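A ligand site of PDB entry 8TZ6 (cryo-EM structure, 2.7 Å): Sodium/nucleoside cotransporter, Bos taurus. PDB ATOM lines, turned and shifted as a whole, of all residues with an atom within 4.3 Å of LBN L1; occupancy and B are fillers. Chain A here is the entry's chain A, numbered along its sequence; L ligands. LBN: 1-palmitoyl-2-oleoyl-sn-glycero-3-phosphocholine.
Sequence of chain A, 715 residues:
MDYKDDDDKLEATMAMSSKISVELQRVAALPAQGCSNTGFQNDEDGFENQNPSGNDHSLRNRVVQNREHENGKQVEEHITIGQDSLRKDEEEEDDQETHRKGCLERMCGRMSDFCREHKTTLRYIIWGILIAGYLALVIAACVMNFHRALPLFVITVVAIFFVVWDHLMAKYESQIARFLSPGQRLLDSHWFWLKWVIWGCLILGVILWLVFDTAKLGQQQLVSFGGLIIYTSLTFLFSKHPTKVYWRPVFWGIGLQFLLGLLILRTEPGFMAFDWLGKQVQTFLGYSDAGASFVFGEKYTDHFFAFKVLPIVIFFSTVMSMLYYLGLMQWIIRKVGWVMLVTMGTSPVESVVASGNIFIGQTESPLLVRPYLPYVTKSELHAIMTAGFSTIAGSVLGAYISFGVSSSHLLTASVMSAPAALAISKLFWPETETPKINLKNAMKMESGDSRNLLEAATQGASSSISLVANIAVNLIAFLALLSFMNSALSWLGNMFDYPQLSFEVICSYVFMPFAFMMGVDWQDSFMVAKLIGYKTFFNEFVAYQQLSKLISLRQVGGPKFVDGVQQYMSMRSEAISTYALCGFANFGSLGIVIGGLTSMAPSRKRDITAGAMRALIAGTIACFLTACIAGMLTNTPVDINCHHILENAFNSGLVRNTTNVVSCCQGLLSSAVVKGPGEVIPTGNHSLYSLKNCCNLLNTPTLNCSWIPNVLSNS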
ATOM      1  N   TRP A 191      12.051  -2.918  10.931  1.00  0.00           N
ATOM      2  CA  TRP A 191      13.305  -2.641  10.224  1.00  0.00           C
ATOM      3  C   TRP A 191      13.819  -1.247  10.516  1.00  0.00           C
ATOM      4  O   TRP A 191      15.038  -1.039  10.649  1.00  0.00           O
ATOM      5  CB  TRP A 191      13.092  -2.835   8.726  1.00  0.00           C
ATOM      6  CG  TRP A 191      14.232  -2.370   7.884  1.00  0.00           C
ATOM      7  CD1 TRP A 191      14.284  -1.234   7.138  1.00  0.00           C
ATOM      8  CD2 TRP A 191      15.490  -3.033   7.702  1.00  0.00           C
ATOM      9  NE1 TRP A 191      15.498  -1.139   6.490  1.00  0.00           N
ATOM     10  CE2 TRP A 191      16.254  -2.233   6.821  1.00  0.00           C
ATOM     11  CE3 TRP A 191      16.041  -4.221   8.184  1.00  0.00           C
ATOM     12  CZ2 TRP A 191      17.541  -2.583   6.427  1.00  0.00           C
ATOM     13  CZ3 TRP A 191      17.319  -4.567   7.787  1.00  0.00           C
ATOM     14  CH2 TRP A 191      18.053  -3.750   6.921  1.00  0.00           C
ATOM     15  N   ILE A 198      21.723  -4.230  12.942  1.00  0.00           N
ATOM     16  CA  ILE A 198      22.340  -5.205  12.044  1.00  0.00           C
ATOM     17  C   ILE A 198      23.608  -4.634  11.436  1.00  0.00           C
ATOM     18  O   ILE A 198      24.655  -5.299  11.370  1.00  0.00           O
ATOM     19  CB  ILE A 198      21.345  -5.658  10.967  1.00  0.00           C
ATOM     20  CG1 ILE A 198      20.180  -6.411  11.630  1.00  0.00           C
ATOM     21  CG2 ILE A 198      22.039  -6.540   9.943  1.00  0.00           C
ATOM     22  CD1 ILE A 198      19.082  -6.823  10.669  1.00  0.00           C
ATOM     23  N   TRP A 199      23.546  -3.380  10.969  1.00  0.00           N
ATOM     24  CA  TRP A 199      24.717  -2.757  10.349  1.00  0.00           C
ATOM     25  C   TRP A 199      25.861  -2.612  11.353  1.00  0.00           C
ATOM     26  O   TRP A 199      27.026  -2.861  11.010  1.00  0.00           O
ATOM     27  CB  TRP A 199      24.327  -1.407   9.761  1.00  0.00           C
ATOM     28  CG  TRP A 199      23.347  -1.493   8.636  1.00  0.00           C
ATOM     29  CD1 TRP A 199      22.956  -2.627   7.978  1.00  0.00           C
ATOM     30  CD2 TRP A 199      22.631  -0.419   8.034  1.00  0.00           C
ATOM     31  NE1 TRP A 199      22.041  -2.312   6.998  1.00  0.00           N
ATOM     32  CE2 TRP A 199      21.826  -0.968   7.014  1.00  0.00           C
ATOM     33  CE3 TRP A 199      22.589   0.967   8.250  1.00  0.00           C
ATOM     34  CZ2 TRP A 199      20.991  -0.185   6.224  1.00  0.00           C
ATOM     35  CZ3 TRP A 199      21.757   1.738   7.466  1.00  0.00           C
ATOM     36  CH2 TRP A 199      20.972   1.167   6.456  1.00  0.00           C
ATOM     37  N   LEU A 202      27.504  -5.971  11.848  1.00  0.00           N
ATOM     38  CA  LEU A 202      28.352  -6.336  10.719  1.00  0.00           C
ATOM     39  C   LEU A 202      29.665  -5.555  10.744  1.00  0.00           C
ATOM     40  O   LEU A 202      30.739  -6.115  10.502  1.00  0.00           O
ATOM     41  CB  LEU A 202      27.612  -6.103   9.409  1.00  0.00           C
ATOM     42  CG  LEU A 202      26.439  -7.045   9.138  1.00  0.00           C
ATOM     43  CD1 LEU A 202      25.628  -6.548   7.954  1.00  0.00           C
ATOM     44  CD2 LEU A 202      26.930  -8.458   8.884  1.00  0.00           C
ATOM     45  N   GLY A 205      31.890  -6.917  13.386  1.00  0.00           N
ATOM     46  CA  GLY A 205      32.471  -8.179  12.954  1.00  0.00           C
ATOM     47  C   GLY A 205      33.624  -7.971  11.993  1.00  0.00           C
ATOM     48  O   GLY A 205      34.654  -8.643  12.098  1.00  0.00           O
ATOM     49  N   VAL A 206      33.482  -7.031  11.058  1.00  0.00           N
ATOM     50  CA  VAL A 206      34.576  -6.721  10.137  1.00  0.00           C
ATOM     51  C   VAL A 206      35.796  -6.247  10.920  1.00  0.00           C
ATOM     52  O   VAL A 206      36.933  -6.683  10.671  1.00  0.00           O
ATOM     53  CB  VAL A 206      34.138  -5.687   9.093  1.00  0.00           C
ATOM     54  CG1 VAL A 206      35.325  -5.230   8.276  1.00  0.00           C
ATOM     55  CG2 VAL A 206      33.061  -6.254   8.198  1.00  0.00           C
ATOM     56  N   TRP A 209      37.423  -9.136  12.812  1.00  0.00           N
ATOM     57  CA  TRP A 209      38.131 -10.024  11.902  1.00  0.00           C
ATOM     58  C   TRP A 209      39.459  -9.418  11.500  1.00  0.00           C
ATOM     59  O   TRP A 209      40.510 -10.074  11.563  1.00  0.00           O
ATOM     60  CB  TRP A 209      37.294 -10.323  10.668  1.00  0.00           C
ATOM     61  CG  TRP A 209      37.987 -11.236   9.715  1.00  0.00           C
ATOM     62  CD1 TRP A 209      38.667 -10.871   8.594  1.00  0.00           C
ATOM     63  CD2 TRP A 209      38.098 -12.658   9.818  1.00  0.00           C
ATOM     64  NE1 TRP A 209      39.189 -11.994   7.983  1.00  0.00           N
ATOM     65  CE2 TRP A 209      38.854 -13.090   8.713  1.00  0.00           C
ATOM     66  CE3 TRP A 209      37.624 -13.600  10.731  1.00  0.00           C
ATOM     67  CZ2 TRP A 209      39.148 -14.435   8.495  1.00  0.00           C
ATOM     68  CZ3 TRP A 209      37.916 -14.928  10.516  1.00  0.00           C
ATOM     69  CH2 TRP A 209      38.674 -15.336   9.410  1.00  0.00           C
ATOM     70  N   TYR A 246      22.705   2.631  -5.911  1.00  0.00           N
ATOM     71  CA  TYR A 246      21.992   1.718  -5.020  1.00  0.00           C
ATOM     72  C   TYR A 246      23.044   0.811  -4.373  1.00  0.00           C
ATOM     73  O   TYR A 246      23.614  -0.056  -5.045  1.00  0.00           O
ATOM     74  CB  TYR A 246      20.945   0.930  -5.805  1.00  0.00           C
ATOM     75  CG  TYR A 246      20.056   0.021  -5.002  1.00  0.00           C
ATOM     76  CD1 TYR A 246      19.536   0.424  -3.775  1.00  0.00           C
ATOM     77  CD2 TYR A 246      19.699  -1.234  -5.477  1.00  0.00           C
ATOM     78  CE1 TYR A 246      18.712  -0.405  -3.036  1.00  0.00           C
ATOM     79  CE2 TYR A 246      18.874  -2.067  -4.747  1.00  0.00           C
ATOM     80  CZ  TYR A 246      18.388  -1.656  -3.536  1.00  0.00           C
ATOM     81  OH  TYR A 246      17.555  -2.488  -2.817  1.00  0.00           O
ATOM     82  N   ARG A 248      22.971  -1.525  -1.968  1.00  0.00           N
ATOM     83  CA  ARG A 248      22.725  -2.899  -1.547  1.00  0.00           C
ATOM     84  C   ARG A 248      23.506  -3.902  -2.368  1.00  0.00           C
ATOM     85  O   ARG A 248      24.222  -4.742  -1.783  1.00  0.00           O
ATOM     86  CB  ARG A 248      21.213  -3.167  -1.612  1.00  0.00           C
ATOM     87  CG  ARG A 248      20.794  -4.578  -1.249  1.00  0.00           C
ATOM     88  CD  ARG A 248      19.351  -4.803  -1.604  1.00  0.00           C
ATOM     89  NE  ARG A 248      18.887  -6.140  -1.266  1.00  0.00           N
ATOM     90  CZ  ARG A 248      17.712  -6.646  -1.631  1.00  0.00           C
ATOM     91  NH1 ARG A 248      16.869  -5.955  -2.375  1.00  0.00           N
ATOM     92  NH2 ARG A 248      17.393  -7.873  -1.238  1.00  0.00           N
ATOM     93  N   PHE A 251      27.570  -3.935  -1.470  1.00  0.00           N
ATOM     94  CA  PHE A 251      27.922  -4.572  -0.219  1.00  0.00           C
ATOM     95  C   PHE A 251      27.599  -6.063  -0.243  1.00  0.00           C
ATOM     96  O   PHE A 251      28.379  -6.876   0.250  1.00  0.00           O
ATOM     97  CB  PHE A 251      27.192  -3.890   0.939  1.00  0.00           C
ATOM     98  CG  PHE A 251      27.616  -2.476   1.166  1.00  0.00           C
ATOM     99  CD1 PHE A 251      28.943  -2.103   1.092  1.00  0.00           C
ATOM    100  CD2 PHE A 251      26.672  -1.498   1.443  1.00  0.00           C
ATOM    101  CE1 PHE A 251      29.325  -0.788   1.302  1.00  0.00           C
ATOM    102  CE2 PHE A 251      27.049  -0.191   1.657  1.00  0.00           C
ATOM    103  CZ  PHE A 251      28.378   0.166   1.580  1.00  0.00           C
ATOM    104  N   TRP A 252      26.456  -6.428  -0.812  1.00  0.00           N
ATOM    105  CA  TRP A 252      26.096  -7.841  -0.840  1.00  0.00           C
ATOM    106  C   TRP A 252      27.057  -8.656  -1.691  1.00  0.00           C
ATOM    107  O   TRP A 252      27.431  -9.766  -1.311  1.00  0.00           O
ATOM    108  CB  TRP A 252      24.659  -8.015  -1.322  1.00  0.00           C
ATOM    109  CG  TRP A 252      23.696  -8.167  -0.191  1.00  0.00           C
ATOM    110  CD1 TRP A 252      22.780  -7.251   0.240  1.00  0.00           C
ATOM    111  CD2 TRP A 252      23.568  -9.298   0.665  1.00  0.00           C
ATOM    112  NE1 TRP A 252      22.082  -7.752   1.305  1.00  0.00           N
ATOM    113  CE2 TRP A 252      22.544  -9.004   1.586  1.00  0.00           C
ATOM    114  CE3 TRP A 252      24.209 -10.545   0.739  1.00  0.00           C
ATOM    115  CZ2 TRP A 252      22.151  -9.915   2.572  1.00  0.00           C
ATOM    116  CZ3 TRP A 252      23.810 -11.432   1.713  1.00  0.00           C
ATOM    117  CH2 TRP A 252      22.794 -11.110   2.620  1.00  0.00           C
ATOM    118  N   GLY A 255      30.314  -9.010   0.231  1.00  0.00           N
ATOM    119  CA  GLY A 255      30.126  -9.956   1.309  1.00  0.00           C
ATOM    120  C   GLY A 255      30.041 -11.393   0.841  1.00  0.00           C
ATOM    121  O   GLY A 255      30.558 -12.294   1.494  1.00  0.00           O
ATOM    122  N   PHE A 258      33.500 -12.488   0.156  1.00  0.00           N
ATOM    123  CA  PHE A 258      34.217 -12.750   1.403  1.00  0.00           C
ATOM    124  C   PHE A 258      33.797 -14.085   2.019  1.00  0.00           C
ATOM    125  O   PHE A 258      34.637 -14.844   2.495  1.00  0.00           O
ATOM    126  CB  PHE A 258      33.990 -11.604   2.378  1.00  0.00           C
ATOM    127  CG  PHE A 258      34.850 -11.674   3.605  1.00  0.00           C
ATOM    128  CD1 PHE A 258      36.207 -11.436   3.520  1.00  0.00           C
ATOM    129  CD2 PHE A 258      34.296 -11.953   4.837  1.00  0.00           C
ATOM    130  CE1 PHE A 258      37.004 -11.499   4.644  1.00  0.00           C
ATOM    131  CE2 PHE A 258      35.088 -12.023   5.965  1.00  0.00           C
ATOM    132  CZ  PHE A 258      36.437 -11.785   5.869  1.00  0.00           C
ATOM    133  N   LEU A 259      32.497 -14.374   2.006  1.00  0.00           N
ATOM    134  CA  LEU A 259      32.014 -15.638   2.565  1.00  0.00           C
ATOM    135  C   LEU A 259      32.528 -16.824   1.762  1.00  0.00           C
ATOM    136  O   LEU A 259      32.949 -17.838   2.349  1.00  0.00           O
ATOM    137  CB  LEU A 259      30.495 -15.641   2.615  1.00  0.00           C
ATOM    138  CG  LEU A 259      29.835 -14.638   3.556  1.00  0.00           C
ATOM    139  CD1 LEU A 259      28.330 -14.732   3.449  1.00  0.00           C
ATOM    140  CD2 LEU A 259      30.281 -14.851   4.984  1.00  0.00           C
HETATM  141  C1  LBN L   1      18.091  -3.531   2.811  1.00  0.00           C
HETATM  142  P1  LBN L   1      16.844  -2.697   0.640  1.00  0.00           P
HETATM  143  C2  LBN L   1      19.395  -4.234   3.196  1.00  0.00           C
HETATM  144  C3  LBN L   1      19.174  -5.740   3.290  1.00  0.00           C
HETATM  145  C5  LBN L   1      28.439 -10.772   4.067  1.00  0.00           C
HETATM  146  O1  LBN L   1      17.787  -3.807   1.468  1.00  0.00           O
HETATM  147  C8  LBN L   1      28.841 -10.319   5.477  1.00  0.00           C
HETATM  148  O2  LBN L   1      17.580  -1.383   0.566  1.00  0.00           O
HETATM  149  C11 LBN L   1      30.274 -10.805   5.818  1.00  0.00           C
HETATM  150  O3  LBN L   1      16.557  -3.207  -0.744  1.00  0.00           O
HETATM  151  C14 LBN L   1      30.798 -10.144   7.100  1.00  0.00           C
HETATM  152  O4  LBN L   1      15.424  -2.484   1.440  1.00  0.00           O
HETATM  153  C17 LBN L   1      32.180 -10.657   7.523  1.00  0.00           C
HETATM  154  C20 LBN L   1      32.481 -10.335   8.978  1.00  0.00           C
HETATM  155  C22 LBN L   1      33.781 -10.969   9.439  1.00  0.00           C
HETATM  156  C23 LBN L   1      33.755 -12.481   9.590  1.00  0.00           C
HETATM  157  C24 LBN L   1      32.437 -13.052  10.075  1.00  0.00           C
HETATM  158  C25 LBN L   1      20.174  -6.453   5.316  1.00  0.00           C
HETATM  159  O5  LBN L   1      18.992  -6.079   4.647  1.00  0.00           O
HETATM  160  C26 LBN L   1      20.865  -7.784   4.984  1.00  0.00           C
HETATM  161  O6  LBN L   1      20.630  -5.739   6.137  1.00  0.00           O
HETATM  162  C27 LBN L   1      21.470  -8.462   6.228  1.00  0.00           C
HETATM  163  C28 LBN L   1      22.333  -9.678   5.869  1.00  0.00           C
HETATM  164  C29 LBN L   1      23.025 -10.300   7.084  1.00  0.00           C
HETATM  165  C30 LBN L   1      24.020 -11.392   6.684  1.00  0.00           C
HETATM  166  C31 LBN L   1      24.525 -12.221   7.882  1.00  0.00           C
HETATM  167  C34 LBN L   1      21.128  -2.785   2.479  1.00  0.00           C
HETATM  168  O7  LBN L   1      20.392  -3.973   2.222  1.00  0.00           O
HETATM  169  C35 LBN L   1      22.509  -2.880   3.195  1.00  0.00           C
HETATM  170  O8  LBN L   1      20.692  -1.726   2.171  1.00  0.00           O
HETATM  171  C36 LBN L   1      23.474  -3.884   2.529  1.00  0.00           C
HETATM  172  C37 LBN L   1      23.707  -5.120   3.408  1.00  0.00           C
HETATM  173  C38 LBN L   1      25.007  -5.873   3.058  1.00  0.00           C
HETATM  174  C39 LBN L   1      25.129  -7.164   3.878  1.00  0.00           C
HETATM  175  C40 LBN L   1      26.348  -8.004   3.505  1.00  0.00           C
HETATM  176  C41 LBN L   1      26.321  -9.383   4.204  1.00  0.00           C
HETATM  177  C42 LBN L   1      27.296 -10.354   3.487  1.00  0.00           C
HETATM  178  C1  LBN L   2      21.726   4.919   0.899  1.00  0.00           C
HETATM  179  P1  LBN L   2      20.447   3.185  -0.629  1.00  0.00           P
HETATM  180  C2  LBN L   2      22.780   3.954   1.462  1.00  0.00           C
HETATM  181  C3  LBN L   2      23.971   4.732   1.960  1.00  0.00           C
HETATM  182  C5  LBN L   2      29.747  -3.995   5.150  1.00  0.00           C
HETATM  183  O1  LBN L   2      20.532   4.207   0.681  1.00  0.00           O
HETATM  184  C8  LBN L   2      29.250  -5.352   4.616  1.00  0.00           C
HETATM  185  O2  LBN L   2      21.261   1.943  -0.349  1.00  0.00           O
HETATM  186  C11 LBN L   2      30.236  -5.850   3.529  1.00  0.00           C
HETATM  187  O3  LBN L   2      20.997   3.889  -1.849  1.00  0.00           O
HETATM  188  C14 LBN L   2      31.295  -6.802   4.098  1.00  0.00           C
HETATM  189  O4  LBN L   2      18.882   2.771  -0.900  1.00  0.00           O
HETATM  190  C17 LBN L   2      32.424  -7.083   3.090  1.00  0.00           C
HETATM  191  C20 LBN L   2      33.733  -7.383   3.799  1.00  0.00           C
HETATM  192  C22 LBN L   2      34.895  -7.509   2.826  1.00  0.00           C
HETATM  193  C23 LBN L   2      36.250  -7.739   3.476  1.00  0.00           C
HETATM  194  C24 LBN L   2      36.225  -7.773   5.002  1.00  0.00           C
HETATM  195  C25 LBN L   2      26.304   4.900   1.693  1.00  0.00           C
HETATM  196  O5  LBN L   2      25.121   4.238   1.327  1.00  0.00           O
HETATM  197  C26 LBN L   2      27.243   4.242   2.720  1.00  0.00           C
HETATM  198  O6  LBN L   2      26.584   5.948   1.233  1.00  0.00           O
HETATM  199  C27 LBN L   2      28.680   4.067   2.202  1.00  0.00           C
HETATM  200  C28 LBN L   2      29.700   3.948   3.350  1.00  0.00           C
HETATM  201  C29 LBN L   2      29.395   2.740   4.248  1.00  0.00           C
HETATM  202  C30 LBN L   2      30.663   2.006   4.704  1.00  0.00           C
HETATM  203  C31 LBN L   2      30.370   0.982   5.822  1.00  0.00           C
HETATM  204  C34 LBN L   2      22.537   1.820   2.496  1.00  0.00           C
HETATM  205  O7  LBN L   2      22.222   3.209   2.536  1.00  0.00           O
HETATM  206  C35 LBN L   2      23.939   1.335   2.949  1.00  0.00           C
HETATM  207  O8  LBN L   2      21.728   1.034   2.108  1.00  0.00           O
HETATM  208  C36 LBN L   2      24.229   1.651   4.429  1.00  0.00           C
HETATM  209  C37 LBN L   2      25.554   1.043   4.900  1.00  0.00           C
HETATM  210  C38 LBN L   2      25.350  -0.280   5.663  1.00  0.00           C
HETATM  211  C39 LBN L   2      26.528  -1.241   5.441  1.00  0.00           C
HETATM  212  C40 LBN L   2      26.719  -2.248   6.576  1.00  0.00           C
HETATM  213  C41 LBN L   2      27.446  -3.515   6.078  1.00  0.00           C
HETATM  214  C42 LBN L   2      28.921  -3.158   5.819  1.00  0.00           C
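Trp 191 touches LBN L1 (CH2 to O6, 3.3 Å).
Trp 199 touches LBN L1 (NE1 to O6, 3.8 Å).
O of Gly 205 touches C22 of LBN L1 (3.6 Å).
CB of Trp 209 touches C22 of LBN L1, at 3.8 Å.
CB of Phe 251 touches C38 of LBN L1, 3.6 Å away.
Trp 252 touches LBN L1 (CZ2 to C28, 3.3 Å).
Gly 255 touches LBN L1 (CA to C5, 3.3 Å).
CE2 of Phe 258 touches C17 of LBN L1, 3.6 Å away.
Hydrophobic or aromatic side chains that line LBN L1: Trp 191, Trp 209, Tyr 246, Phe 251, Trp 252 and Phe 258.
Ten residues have an atom within 4 Å of LBN L1: Trp 191, Trp 199, Gly 205, Trp 209, Tyr 246, Arg 248, Phe 251, Trp 252, Gly 255 and Phe 258.
OH of Tyr 246 is in hydrogen-bond range of O3 of LBN L1 (2.4 Å).
O3 of LBN L1 lies within salt-bridge range of NH1 of Arg 248, 3.2 Å away.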
